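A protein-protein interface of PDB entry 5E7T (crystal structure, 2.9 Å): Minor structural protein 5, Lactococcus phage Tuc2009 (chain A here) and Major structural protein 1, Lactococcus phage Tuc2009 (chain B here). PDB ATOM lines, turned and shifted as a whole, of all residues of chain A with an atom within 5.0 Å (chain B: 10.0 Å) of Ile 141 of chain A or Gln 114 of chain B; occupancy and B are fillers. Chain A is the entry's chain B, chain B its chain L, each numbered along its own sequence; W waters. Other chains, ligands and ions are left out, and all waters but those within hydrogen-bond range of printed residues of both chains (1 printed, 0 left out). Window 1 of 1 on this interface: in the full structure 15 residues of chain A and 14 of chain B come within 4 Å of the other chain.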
ATOM      1  N   MET A  88      -7.511 -20.957   0.123  1.00  0.00           N
ATOM      2  CA  MET A  88      -6.369 -20.205  -0.363  1.00  0.00           C
ATOM      3  C   MET A  88      -6.683 -19.706  -1.746  1.00  0.00           C
ATOM      4  O   MET A  88      -7.275 -20.440  -2.520  1.00  0.00           O
ATOM      5  CB  MET A  88      -5.117 -21.066  -0.365  1.00  0.00           C
ATOM      6  CG  MET A  88      -4.610 -21.364   1.006  1.00  0.00           C
ATOM      7  SD  MET A  88      -3.070 -22.283   0.891  1.00  0.00           S
ATOM      8  CE  MET A  88      -1.884 -20.889   0.802  1.00  0.00           C
ATOM      9  N   SER A  89      -6.329 -18.449  -2.043  1.00  0.00           N
ATOM     10  CA  SER A  89      -6.550 -17.741  -3.325  1.00  0.00           C
ATOM     11  C   SER A  89      -5.287 -16.919  -3.614  1.00  0.00           C
ATOM     12  O   SER A  89      -4.707 -16.365  -2.680  1.00  0.00           O
ATOM     13  CB  SER A  89      -7.773 -16.823  -3.254  1.00  0.00           C
ATOM     14  OG  SER A  89      -8.317 -16.703  -1.945  1.00  0.00           O
ATOM     15  N   VAL A  90      -4.818 -16.883  -4.883  1.00  0.00           N
ATOM     16  CA  VAL A  90      -3.593 -16.171  -5.256  1.00  0.00           C
ATOM     17  C   VAL A  90      -3.569 -15.910  -6.756  1.00  0.00           C
ATOM     18  O   VAL A  90      -4.093 -16.726  -7.523  1.00  0.00           O
ATOM     19  CB  VAL A  90      -2.323 -16.939  -4.767  1.00  0.00           C
ATOM     20  CG1 VAL A  90      -2.177 -18.305  -5.436  1.00  0.00           C
ATOM     21  CG2 VAL A  90      -1.061 -16.109  -4.930  1.00  0.00           C
ATOM     22  N   VAL A  92      -0.983 -15.370  -9.896  1.00  0.00           N
ATOM     23  CA  VAL A  92       0.341 -15.867 -10.218  1.00  0.00           C
ATOM     24  C   VAL A  92       0.716 -15.589 -11.687  1.00  0.00           C
ATOM     25  O   VAL A  92      -0.144 -15.676 -12.571  1.00  0.00           O
ATOM     26  CB  VAL A  92       0.332 -17.359  -9.801  1.00  0.00           C
ATOM     27  CG1 VAL A  92       0.699 -18.314 -10.920  1.00  0.00           C
ATOM     28  CG2 VAL A  92       1.174 -17.578  -8.565  1.00  0.00           C
ATOM     29  N   ILE A 125      -1.991 -25.195  -1.726  1.00  0.00           N
ATOM     30  CA  ILE A 125      -2.458 -24.775  -3.039  1.00  0.00           C
ATOM     31  C   ILE A 125      -1.418 -25.119  -4.093  1.00  0.00           C
ATOM     32  O   ILE A 125      -0.287 -24.642  -4.030  1.00  0.00           O
ATOM     33  CB  ILE A 125      -2.939 -23.299  -3.094  1.00  0.00           C
ATOM     34  CG1 ILE A 125      -3.628 -22.992  -4.443  1.00  0.00           C
ATOM     35  CG2 ILE A 125      -1.819 -22.276  -2.732  1.00  0.00           C
ATOM     36  CD1 ILE A 125      -4.372 -21.777  -4.438  1.00  0.00           C
ATOM     37  N   ASP A 126      -1.804 -25.979  -5.048  1.00  0.00           N
ATOM     38  CA  ASP A 126      -0.953 -26.408  -6.150  1.00  0.00           C
ATOM     39  C   ASP A 126      -0.785 -25.243  -7.125  1.00  0.00           C
ATOM     40  O   ASP A 126      -1.733 -24.495  -7.381  1.00  0.00           O
ATOM     41  CB  ASP A 126      -1.598 -27.586  -6.894  1.00  0.00           C
ATOM     42  CG  ASP A 126      -1.342 -29.002  -6.396  1.00  0.00           C
ATOM     43  OD1 ASP A 126      -0.473 -29.179  -5.496  1.00  0.00           O
ATOM     44  OD2 ASP A 126      -1.990 -29.950  -6.938  1.00  0.00           O
ATOM     45  N   LEU A 127       0.428 -25.096  -7.659  1.00  0.00           N
ATOM     46  CA  LEU A 127       0.747 -24.063  -8.630  1.00  0.00           C
ATOM     47  C   LEU A 127       0.930 -24.727  -9.990  1.00  0.00           C
ATOM     48  O   LEU A 127       1.121 -25.953 -10.010  1.00  0.00           O
ATOM     49  CB  LEU A 127       1.959 -23.244  -8.183  1.00  0.00           C
ATOM     50  CG  LEU A 127       1.765 -22.418  -6.909  1.00  0.00           C
ATOM     51  CD1 LEU A 127       2.906 -21.464  -6.718  1.00  0.00           C
ATOM     52  CD2 LEU A 127       0.458 -21.661  -6.919  1.00  0.00           C
ATOM     53  N   PRO A 128       0.750 -23.991 -11.131  1.00  0.00           N
ATOM     54  CA  PRO A 128       0.778 -24.644 -12.449  1.00  0.00           C
ATOM     55  C   PRO A 128       2.035 -25.417 -12.759  1.00  0.00           C
ATOM     56  O   PRO A 128       3.103 -24.836 -12.787  1.00  0.00           O
ATOM     57  CB  PRO A 128       0.548 -23.483 -13.421  1.00  0.00           C
ATOM     58  CG  PRO A 128      -0.247 -22.519 -12.646  1.00  0.00           C
ATOM     59  CD  PRO A 128       0.421 -22.559 -11.289  1.00  0.00           C
ATOM     60  N   ILE A 139      -2.764 -15.600 -13.536  1.00  0.00           N
ATOM     61  CA  ILE A 139      -3.628 -16.735 -13.319  1.00  0.00           C
ATOM     62  C   ILE A 139      -4.107 -16.658 -11.860  1.00  0.00           C
ATOM     63  O   ILE A 139      -3.270 -16.577 -10.941  1.00  0.00           O
ATOM     64  CB  ILE A 139      -2.889 -18.078 -13.604  1.00  0.00           C
ATOM     65  CG1 ILE A 139      -2.191 -18.096 -14.972  1.00  0.00           C
ATOM     66  CG2 ILE A 139      -3.830 -19.275 -13.441  1.00  0.00           C
ATOM     67  CD1 ILE A 139      -0.995 -19.091 -15.070  1.00  0.00           C
ATOM     68  N   ARG A 140      -5.437 -16.689 -11.645  1.00  0.00           N
ATOM     69  CA  ARG A 140      -6.033 -16.751 -10.307  1.00  0.00           C
ATOM     70  C   ARG A 140      -6.194 -18.235  -9.966  1.00  0.00           C
ATOM     71  O   ARG A 140      -6.822 -18.972 -10.734  1.00  0.00           O
ATOM     72  CB  ARG A 140      -7.407 -16.096 -10.283  1.00  0.00           C
ATOM     73  CG  ARG A 140      -8.107 -16.280  -8.953  1.00  0.00           C
ATOM     74  CD  ARG A 140      -9.080 -15.181  -8.607  1.00  0.00           C
ATOM     75  NE  ARG A 140     -10.303 -15.769  -8.073  1.00  0.00           N
ATOM     76  CZ  ARG A 140     -10.679 -15.711  -6.802  1.00  0.00           C
ATOM     77  NH1 ARG A 140      -9.957 -15.029  -5.920  1.00  0.00           N
ATOM     78  NH2 ARG A 140     -11.799 -16.309  -6.408  1.00  0.00           N
ATOM     79  N   ILE A 141      -5.623 -18.685  -8.838  1.00  0.00           N
ATOM     80  CA  ILE A 141      -5.698 -20.093  -8.430  1.00  0.00           C
ATOM     81  C   ILE A 141      -6.317 -20.173  -7.044  1.00  0.00           C
ATOM     82  O   ILE A 141      -5.887 -19.453  -6.153  1.00  0.00           O
ATOM     83  CB  ILE A 141      -4.302 -20.770  -8.522  1.00  0.00           C
ATOM     84  CG1 ILE A 141      -3.664 -20.539  -9.907  1.00  0.00           C
ATOM     85  CG2 ILE A 141      -4.403 -22.265  -8.235  1.00  0.00           C
ATOM     86  CD1 ILE A 141      -2.245 -20.619  -9.936  1.00  0.00           C
ATOM     87  N   THR A 142      -7.354 -21.007  -6.868  1.00  0.00           N
ATOM     88  CA  THR A 142      -8.065 -21.186  -5.590  1.00  0.00           C
ATOM     89  C   THR A 142      -8.121 -22.661  -5.183  1.00  0.00           C
ATOM     90  O   THR A 142      -8.135 -23.541  -6.050  1.00  0.00           O
ATOM     91  CB  THR A 142      -9.466 -20.528  -5.616  1.00  0.00           C
ATOM     92  OG1 THR A 142     -10.411 -21.366  -6.282  1.00  0.00           O
ATOM     93  CG2 THR A 142      -9.471 -19.141  -6.238  1.00  0.00           C
ATOM     94  N   GLN A 143      -8.148 -22.935  -3.867  1.00  0.00           N
ATOM     95  CA  GLN A 143      -8.211 -24.295  -3.311  1.00  0.00           C
ATOM     96  C   GLN A 143      -8.681 -24.267  -1.856  1.00  0.00           C
ATOM     97  O   GLN A 143      -8.133 -23.517  -1.045  1.00  0.00           O
ATOM     98  CB  GLN A 143      -6.837 -24.972  -3.408  1.00  0.00           C
ATOM     99  CG  GLN A 143      -6.725 -26.365  -2.802  1.00  0.00           C
ATOM    100  CD  GLN A 143      -7.373 -27.436  -3.618  1.00  0.00           C
ATOM    101  OE1 GLN A 143      -6.913 -27.788  -4.715  1.00  0.00           O
ATOM    102  NE2 GLN A 143      -8.400 -28.042  -3.049  1.00  0.00           N
ATOM    103  N   GLU B 103     -13.224 -15.027 -19.968  1.00  0.00           N
ATOM    104  CA  GLU B 103     -12.812 -15.392 -18.627  1.00  0.00           C
ATOM    105  C   GLU B 103     -12.985 -16.908 -18.574  1.00  0.00           C
ATOM    106  O   GLU B 103     -14.116 -17.396 -18.532  1.00  0.00           O
ATOM    107  CB  GLU B 103     -13.657 -14.660 -17.561  1.00  0.00           C
ATOM    108  CG  GLU B 103     -13.391 -15.138 -16.140  1.00  0.00           C
ATOM    109  CD  GLU B 103     -13.821 -14.222 -15.023  1.00  0.00           C
ATOM    110  OE1 GLU B 103     -13.063 -13.276 -14.711  1.00  0.00           O
ATOM    111  OE2 GLU B 103     -14.865 -14.507 -14.394  1.00  0.00           O
ATOM    112  N   ILE B 104     -11.874 -17.654 -18.683  1.00  0.00           N
ATOM    113  CA  ILE B 104     -11.895 -19.125 -18.697  1.00  0.00           C
ATOM    114  C   ILE B 104     -11.460 -19.653 -17.346  1.00  0.00           C
ATOM    115  O   ILE B 104     -10.459 -19.173 -16.788  1.00  0.00           O
ATOM    116  CB  ILE B 104     -11.010 -19.717 -19.823  1.00  0.00           C
ATOM    117  CG1 ILE B 104     -11.282 -19.084 -21.210  1.00  0.00           C
ATOM    118  CG2 ILE B 104     -11.097 -21.237 -19.882  1.00  0.00           C
ATOM    119  CD1 ILE B 104     -12.718 -19.152 -21.746  1.00  0.00           C
ATOM    120  N   GLY B 105     -12.196 -20.656 -16.860  1.00  0.00           N
ATOM    121  CA  GLY B 105     -11.906 -21.348 -15.617  1.00  0.00           C
ATOM    122  C   GLY B 105     -11.665 -22.825 -15.829  1.00  0.00           C
ATOM    123  O   GLY B 105     -12.366 -23.455 -16.622  1.00  0.00           O
ATOM    124  N   ILE B 106     -10.673 -23.385 -15.140  1.00  0.00           N
ATOM    125  CA  ILE B 106     -10.359 -24.813 -15.213  1.00  0.00           C
ATOM    126  C   ILE B 106     -10.465 -25.387 -13.809  1.00  0.00           C
ATOM    127  O   ILE B 106      -9.776 -24.914 -12.905  1.00  0.00           O
ATOM    128  CB  ILE B 106      -8.957 -25.053 -15.801  1.00  0.00           C
ATOM    129  CG1 ILE B 106      -8.784 -24.357 -17.171  1.00  0.00           C
ATOM    130  CG2 ILE B 106      -8.652 -26.556 -15.861  1.00  0.00           C
ATOM    131  CD1 ILE B 106      -7.377 -24.310 -17.666  1.00  0.00           C
ATOM    132  N   THR B 107     -11.324 -26.386 -13.616  1.00  0.00           N
ATOM    133  CA  THR B 107     -11.530 -26.998 -12.299  1.00  0.00           C
ATOM    134  C   THR B 107     -11.254 -28.476 -12.335  1.00  0.00           C
ATOM    135  O   THR B 107     -11.469 -29.136 -13.366  1.00  0.00           O
ATOM    136  CB  THR B 107     -12.972 -26.817 -11.799  1.00  0.00           C
ATOM    137  OG1 THR B 107     -13.677 -25.835 -12.565  1.00  0.00           O
ATOM    138  CG2 THR B 107     -13.030 -26.507 -10.322  1.00  0.00           C
ATOM    139  N   THR B 108     -10.820 -29.012 -11.189  1.00  0.00           N
ATOM    140  CA  THR B 108     -10.570 -30.439 -11.043  1.00  0.00           C
ATOM    141  C   THR B 108     -11.411 -30.963  -9.886  1.00  0.00           C
ATOM    142  O   THR B 108     -11.573 -30.247  -8.884  1.00  0.00           O
ATOM    143  CB  THR B 108      -9.065 -30.740 -10.846  1.00  0.00           C
ATOM    144  OG1 THR B 108      -8.571 -30.170  -9.618  1.00  0.00           O
ATOM    145  CG2 THR B 108      -8.209 -30.313 -12.048  1.00  0.00           C
ATOM    146  N   GLY B 111     -10.708 -30.073  -6.274  1.00  0.00           N
ATOM    147  CA  GLY B 111     -11.039 -28.735  -5.800  1.00  0.00           C
ATOM    148  C   GLY B 111     -10.116 -27.607  -6.194  1.00  0.00           C
ATOM    149  O   GLY B 111     -10.163 -26.539  -5.577  1.00  0.00           O
ATOM    150  N   LEU B 112      -9.297 -27.811  -7.232  1.00  0.00           N
ATOM    151  CA  LEU B 112      -8.366 -26.799  -7.706  1.00  0.00           C
ATOM    152  C   LEU B 112      -9.011 -26.072  -8.839  1.00  0.00           C
ATOM    153  O   LEU B 112      -9.439 -26.711  -9.806  1.00  0.00           O
ATOM    154  CB  LEU B 112      -7.043 -27.442  -8.182  1.00  0.00           C
ATOM    155  CG  LEU B 112      -6.004 -26.490  -8.805  1.00  0.00           C
ATOM    156  CD1 LEU B 112      -5.237 -25.759  -7.755  1.00  0.00           C
ATOM    157  CD2 LEU B 112      -5.061 -27.221  -9.751  1.00  0.00           C
ATOM    158  N   THR B 113      -9.062 -24.737  -8.757  1.00  0.00           N
ATOM    159  CA  THR B 113      -9.643 -23.954  -9.846  1.00  0.00           C
ATOM    160  C   THR B 113      -8.626 -22.897 -10.333  1.00  0.00           C
ATOM    161  O   THR B 113      -7.894 -22.339  -9.511  1.00  0.00           O
ATOM    162  CB  THR B 113     -11.080 -23.399  -9.521  1.00  0.00           C
ATOM    163  OG1 THR B 113     -11.160 -21.991  -9.737  1.00  0.00           O
ATOM    164  CG2 THR B 113     -11.589 -23.757  -8.126  1.00  0.00           C
ATOM    165  N   GLN B 114      -8.556 -22.663 -11.677  1.00  0.00           N
ATOM    166  CA  GLN B 114      -7.681 -21.632 -12.270  1.00  0.00           C
ATOM    167  C   GLN B 114      -8.546 -20.723 -13.111  1.00  0.00           C
ATOM    168  O   GLN B 114      -9.384 -21.228 -13.853  1.00  0.00           O
ATOM    169  CB  GLN B 114      -6.569 -22.234 -13.137  1.00  0.00           C
ATOM    170  CG  GLN B 114      -5.532 -22.996 -12.341  1.00  0.00           C
ATOM    171  CD  GLN B 114      -4.600 -23.808 -13.182  1.00  0.00           C
ATOM    172  OE1 GLN B 114      -4.786 -24.013 -14.383  1.00  0.00           O
ATOM    173  NE2 GLN B 114      -3.563 -24.299 -12.541  1.00  0.00           N
ATOM    174  N   ILE B 115      -8.412 -19.396 -12.954  1.00  0.00           N
ATOM    175  CA  ILE B 115      -9.241 -18.427 -13.687  1.00  0.00           C
ATOM    176  C   ILE B 115      -8.354 -17.447 -14.448  1.00  0.00           C
ATOM    177  O   ILE B 115      -7.654 -16.636 -13.835  1.00  0.00           O
ATOM    178  CB  ILE B 115     -10.303 -17.724 -12.793  1.00  0.00           C
ATOM    179  CG1 ILE B 115     -11.260 -18.737 -12.142  1.00  0.00           C
ATOM    180  CG2 ILE B 115     -11.091 -16.680 -13.574  1.00  0.00           C
ATOM    181  CD1 ILE B 115     -11.432 -18.532 -10.675  1.00  0.00           C
ATOM    182  N   TYR B 116      -8.401 -17.557 -15.796  1.00  0.00           N
ATOM    183  CA  TYR B 116      -7.648 -16.798 -16.785  1.00  0.00           C
ATOM    184  C   TYR B 116      -8.542 -15.743 -17.418  1.00  0.00           C
ATOM    185  O   TYR B 116      -9.513 -16.098 -18.082  1.00  0.00           O
ATOM    186  CB  TYR B 116      -7.179 -17.745 -17.890  1.00  0.00           C
ATOM    187  CG  TYR B 116      -6.356 -18.916 -17.410  1.00  0.00           C
ATOM    188  CD1 TYR B 116      -6.959 -20.101 -17.020  1.00  0.00           C
ATOM    189  CD2 TYR B 116      -4.967 -18.868 -17.428  1.00  0.00           C
ATOM    190  CE1 TYR B 116      -6.202 -21.197 -16.619  1.00  0.00           C
ATOM    191  CE2 TYR B 116      -4.201 -19.956 -17.026  1.00  0.00           C
ATOM    192  CZ  TYR B 116      -4.821 -21.117 -16.621  1.00  0.00           C
ATOM    193  OH  TYR B 116      -4.062 -22.171 -16.187  1.00  0.00           O
ATOM    194  N   GLU B 117      -8.203 -14.457 -17.247  1.00  0.00           N
ATOM    195  CA  GLU B 117      -8.964 -13.329 -17.787  1.00  0.00           C
ATOM    196  C   GLU B 117      -8.148 -12.589 -18.844  1.00  0.00           C
ATOM    197  O   GLU B 117      -7.072 -12.059 -18.558  1.00  0.00           O
ATOM    198  CB  GLU B 117      -9.386 -12.394 -16.652  1.00  0.00           C
ATOM    199  CG  GLU B 117     -10.580 -11.524 -16.972  1.00  0.00           C
ATOM    200  CD  GLU B 117     -11.000 -10.537 -15.900  1.00  0.00           C
ATOM    201  OE1 GLU B 117     -11.984  -9.803 -16.145  1.00  0.00           O
ATOM    202  OE2 GLU B 117     -10.347 -10.480 -14.831  1.00  0.00           O
ATOM    203  N   ILE B 137      -5.037 -21.273 -25.177  1.00  0.00           N
ATOM    204  CA  ILE B 137      -4.158 -22.452 -25.082  1.00  0.00           C
ATOM    205  C   ILE B 137      -3.698 -22.723 -23.625  1.00  0.00           C
ATOM    206  O   ILE B 137      -3.362 -21.775 -22.909  1.00  0.00           O
ATOM    207  CB  ILE B 137      -2.976 -22.359 -26.080  1.00  0.00           C
ATOM    208  CG1 ILE B 137      -2.428 -23.770 -26.397  1.00  0.00           C
ATOM    209  CG2 ILE B 137      -1.893 -21.389 -25.599  1.00  0.00           C
ATOM    210  CD1 ILE B 137      -1.553 -23.858 -27.613  1.00  0.00           C
ATOM    211  N   TYR B 138      -3.695 -24.009 -23.200  1.00  0.00           N
ATOM    212  CA  TYR B 138      -3.304 -24.453 -21.862  1.00  0.00           C
ATOM    213  C   TYR B 138      -2.355 -25.592 -21.971  1.00  0.00           C
ATOM    214  O   TYR B 138      -2.643 -26.627 -22.573  1.00  0.00           O
ATOM    215  CB  TYR B 138      -4.516 -24.801 -20.996  1.00  0.00           C
ATOM    216  CG  TYR B 138      -5.486 -23.651 -20.927  1.00  0.00           C
ATOM    217  CD1 TYR B 138      -5.224 -22.545 -20.127  1.00  0.00           C
ATOM    218  CD2 TYR B 138      -6.595 -23.602 -21.767  1.00  0.00           C
ATOM    219  CE1 TYR B 138      -6.057 -21.428 -20.143  1.00  0.00           C
ATOM    220  CE2 TYR B 138      -7.457 -22.507 -21.763  1.00  0.00           C
ATOM    221  CZ  TYR B 138      -7.182 -21.423 -20.946  1.00  0.00           C
ATOM    222  OH  TYR B 138      -7.993 -20.329 -20.957  1.00  0.00           O
ATOM    223  N   SER B 139      -1.271 -25.430 -21.269  1.00  0.00           N
ATOM    224  CA  SER B 139      -0.041 -26.141 -21.316  1.00  0.00           C
ATOM    225  C   SER B 139       0.101 -27.468 -20.592  1.00  0.00           C
ATOM    226  O   SER B 139       0.577 -28.420 -21.242  1.00  0.00           O
ATOM    227  CB  SER B 139       1.045 -25.215 -20.817  1.00  0.00           C
ATOM    228  OG  SER B 139       2.244 -25.418 -21.527  1.00  0.00           O
ATOM    229  N   GLY B 140      -0.141 -27.548 -19.286  1.00  0.00           N
ATOM    230  CA  GLY B 140       0.237 -28.783 -18.597  1.00  0.00           C
ATOM    231  C   GLY B 140      -0.794 -29.805 -18.182  1.00  0.00           C
ATOM    232  O   GLY B 140      -0.759 -30.277 -17.036  1.00  0.00           O
ATOM    233  N   LEU B 141      -1.672 -30.217 -19.116  1.00  0.00           N
ATOM    234  CA  LEU B 141      -2.679 -31.210 -18.748  1.00  0.00           C
ATOM    235  C   LEU B 141      -2.014 -32.575 -18.522  1.00  0.00           C
ATOM    236  O   LEU B 141      -0.976 -32.864 -19.142  1.00  0.00           O
ATOM    237  CB  LEU B 141      -3.896 -31.271 -19.700  1.00  0.00           C
ATOM    238  CG  LEU B 141      -4.665 -29.980 -20.177  1.00  0.00           C
ATOM    239  CD1 LEU B 141      -6.110 -30.304 -20.424  1.00  0.00           C
ATOM    240  CD2 LEU B 141      -4.697 -28.906 -19.180  1.00  0.00           C
ATOM    241  N   TYR B 147     -10.890 -32.630 -15.889  1.00  0.00           N
ATOM    242  CA  TYR B 147     -10.921 -31.180 -15.973  1.00  0.00           C
ATOM    243  C   TYR B 147     -12.309 -30.714 -16.414  1.00  0.00           C
ATOM    244  O   TYR B 147     -12.974 -31.400 -17.190  1.00  0.00           O
ATOM    245  CB  TYR B 147      -9.901 -30.701 -17.011  1.00  0.00           C
ATOM    246  CG  TYR B 147      -8.472 -31.007 -16.653  1.00  0.00           C
ATOM    247  CD1 TYR B 147      -7.761 -30.188 -15.784  1.00  0.00           C
ATOM    248  CD2 TYR B 147      -7.814 -32.098 -17.207  1.00  0.00           C
ATOM    249  CE1 TYR B 147      -6.431 -30.462 -15.456  1.00  0.00           C
ATOM    250  CE2 TYR B 147      -6.483 -32.383 -16.885  1.00  0.00           C
ATOM    251  CZ  TYR B 147      -5.795 -31.562 -16.011  1.00  0.00           C
ATOM    252  OH  TYR B 147      -4.494 -31.847 -15.669  1.00  0.00           O
ATOM    253  N   THR B 148     -12.720 -29.522 -15.946  1.00  0.00           N
ATOM    254  CA  THR B 148     -13.962 -28.855 -16.328  1.00  0.00           C
ATOM    255  C   THR B 148     -13.610 -27.428 -16.735  1.00  0.00           C
ATOM    256  O   THR B 148     -13.246 -26.590 -15.892  1.00  0.00           O
ATOM    257  CB  THR B 148     -15.042 -28.940 -15.234  1.00  0.00           C
ATOM    258  OG1 THR B 148     -15.360 -30.318 -14.944  1.00  0.00           O
ATOM    259  CG2 THR B 148     -16.308 -28.169 -15.608  1.00  0.00           C
ATOM    260  N   PHE B 149     -13.698 -27.161 -18.041  1.00  0.00           N
ATOM    261  CA  PHE B 149     -13.436 -25.849 -18.622  1.00  0.00           C
ATOM    262  C   PHE B 149     -14.759 -25.119 -18.707  1.00  0.00           C
ATOM    263  O   PHE B 149     -15.779 -25.765 -18.904  1.00  0.00           O
ATOM    264  CB  PHE B 149     -12.811 -26.014 -20.016  1.00  0.00           C
ATOM    265  CG  PHE B 149     -11.352 -26.413 -20.014  1.00  0.00           C
ATOM    266  CD1 PHE B 149     -10.949 -27.645 -19.521  1.00  0.00           C
ATOM    267  CD2 PHE B 149     -10.377 -25.545 -20.481  1.00  0.00           C
ATOM    268  CE1 PHE B 149      -9.599 -27.988 -19.473  1.00  0.00           C
ATOM    269  CE2 PHE B 149      -9.024 -25.907 -20.461  1.00  0.00           C
ATOM    270  CZ  PHE B 149      -8.643 -27.117 -19.940  1.00  0.00           C
ATOM    271  N   ASP B 150     -14.766 -23.784 -18.520  1.00  0.00           N
ATOM    272  CA  ASP B 150     -15.983 -22.977 -18.667  1.00  0.00           C
ATOM    273  C   ASP B 150     -15.721 -21.518 -18.981  1.00  0.00           C
ATOM    274  O   ASP B 150     -14.754 -20.969 -18.467  1.00  0.00           O
ATOM    275  CB  ASP B 150     -16.924 -23.100 -17.468  1.00  0.00           C
ATOM    276  CG  ASP B 150     -16.377 -22.552 -16.189  1.00  0.00           C
ATOM    277  OD1 ASP B 150     -15.371 -23.123 -15.674  1.00  0.00           O
ATOM    278  OD2 ASP B 150     -16.997 -21.615 -15.642  1.00  0.00           O
ATOM    279  N   ILE B 151     -16.568 -20.897 -19.847  1.00  0.00           N
ATOM    280  CA  ILE B 151     -16.486 -19.466 -20.133  1.00  0.00           C
ATOM    281  C   ILE B 151     -17.430 -18.790 -19.153  1.00  0.00           C
ATOM    282  O   ILE B 151     -18.635 -18.972 -19.209  1.00  0.00           O
ATOM    283  CB  ILE B 151     -16.623 -19.025 -21.658  1.00  0.00           C
ATOM    284  CG1 ILE B 151     -16.140 -17.538 -21.916  1.00  0.00           C
ATOM    285  CG2 ILE B 151     -17.982 -19.282 -22.221  1.00  0.00           C
ATOM    286  CD1 ILE B 151     -16.932 -16.424 -22.865  1.00  0.00           C
ATOM    287  N   ARG B 152     -16.871 -18.104 -18.184  1.00  0.00           N
ATOM    288  CA  ARG B 152     -17.650 -17.381 -17.190  1.00  0.00           C
ATOM    289  C   ARG B 152     -18.298 -16.176 -17.904  1.00  0.00           C
ATOM    290  O   ARG B 152     -17.617 -15.471 -18.670  1.00  0.00           O
ATOM    291  CB  ARG B 152     -16.759 -17.020 -15.989  1.00  0.00           C
ATOM    292  CG  ARG B 152     -16.100 -18.286 -15.388  1.00  0.00           C
ATOM    293  CD  ARG B 152     -15.097 -18.056 -14.250  1.00  0.00           C
ATOM    294  NE  ARG B 152     -15.221 -19.036 -13.151  1.00  0.00           N
ATOM    295  CZ  ARG B 152     -14.931 -20.339 -13.243  1.00  0.00           C
ATOM    296  NH1 ARG B 152     -14.507 -20.852 -14.387  1.00  0.00           N
ATOM    297  NH2 ARG B 152     -15.082 -21.138 -12.192  1.00  0.00           N
HETATM  298  O   HOH W   1      -2.177 -24.973 -10.156  1.00  0.00           O
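The backbone NH (N) of Ile 115 of chain B is in hydrogen-bond range of the backbone carbonyl oxygen (O) of Arg 140 of chain A, at 2.8 Å.
The backbone NH of Thr 142 of chain A lies within hydrogen-bond range of the backbone carbonyl oxygen of Thr 113 of chain B (3.0 Å).
The backbone carbonyl oxygen (O) of Gly 111 of chain B sits at hydrogen-bond distance from the side-chain amide nitrogen (NE2) of Gln 143 of chain A.
The side-chain amide oxygen (OE1) of Gln 143 of chain A sits at hydrogen-bond distance from the backbone NH (N) of Leu 112 of chain B (3.5 Å).
N of Met 88 of chain A is in hydrogen-bond range of O of Gln 143 of chain A (2.9 Å).
The backbone NH of Ile 141 of chain A is in hydrogen-bond range of the backbone carbonyl oxygen of Val 90 of chain A (2.8 Å).
The backbone NH (N) of Val 92 of chain A sits at hydrogen-bond distance from the backbone carbonyl oxygen (O) of Ile 139 of chain A (2.8 Å).
The backbone carbonyl oxygen of Ile 104 of chain B sits at hydrogen-bond distance from the backbone NH of Tyr 116 of chain B (2.8 Å).
O of Gln 114 of chain B lies within hydrogen-bond range of N of Ile 106 of chain B (2.8 Å).
N of Leu 112 of chain B is in hydrogen-bond range of OG1 of Thr 108 of chain B, at 3.4 Å.
Among the printed residues, pairs that only touch across the chains: Asp 126 of chain A with Leu 112 of chain B (3.7 Å), Pro 128 of chain A with Gln 114 of chain B (3.8 Å), Ile 139 of chain A with Tyr 116 of chain B (3.4 Å), Arg 140 of chain A with Thr 113 of chain B (3.7 Å), Arg 140 of chain A with Gln 114 of chain B (3.2 Å), Ile 141 of chain A with Leu 112 of chain B (3.6 Å), Ile 141 of chain A with Thr 113 of chain B (3.3 Å), Ile 141 of chain A with Gln 114 of chain B (3.9 Å), Thr 142 of chain A with Gly 111 of chain B (3.7 Å) and Thr 142 of chain A with Leu 112 of chain B (3.7 Å).
Printed residues of chain A within 4 Å of Gln 114 of chain B: Pro 128, Arg 140 and Ile 141.
No residue of chain B comes within 4 Å of Ser 89 of chain A.
Thr 142 of chain A touches just these residues of chain B: Gly 111 (3.7 Å), Leu 112 (3.7 Å) and Thr 113 (3.0 Å).
Of the printed residues of chain A, Gly 111 of chain B touches Thr 142 (3.7 Å) and Gln 143 (3.4 Å).
Of the printed residues of chain B, Arg 140 of chain A touches Thr 113, Gln 114 and Ile 115.
Ile 106 of chain B touches none of the printed residues of chain A.
Glu 117 of chain B touches none of the printed residues of chain A.
The nearest residue of chain B that does not touch Ile 141 of chain A is Ile 115 of chain B (5.0 Å).
The nearest residue of chain A that does not touch Gln 114 of chain B is Ile 139 of chain A (4.04 Å).
The nearest printed residue of chain B that does not touch Gln 143 of chain A is Thr 113 of chain B (5.3 Å).
Of the 13 printed residues of chain A, 7 touch a printed residue of chain B.
Printed residues of chain A that touch a printed residue of chain B: Asp 126, Pro 128, Ile 139, Arg 140, Ile 141, Thr 142 and Gln 143.
Printed residues of chain B that touch a printed residue of chain A: Gly 111, Leu 112, Thr 113, Gln 114, Ile 115 and Tyr 116.
Hydrophobic or aromatic side chains of chain B within 4 Å of the printed part of chain A: Leu 112, Ile 115 and Tyr 116.
Among the printed residues, 14 pairs touch across the chains.
Water W1 lies within hydrogen-bond range of the side-chain amide nitrogen of Gln 114 of chain B (2.8 Å), the backbone carbonyl oxygen of Asp 126 of chain A (2.9 Å) and the backbone carbonyl oxygen of Leu 127 of chain A (3.4 Å).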
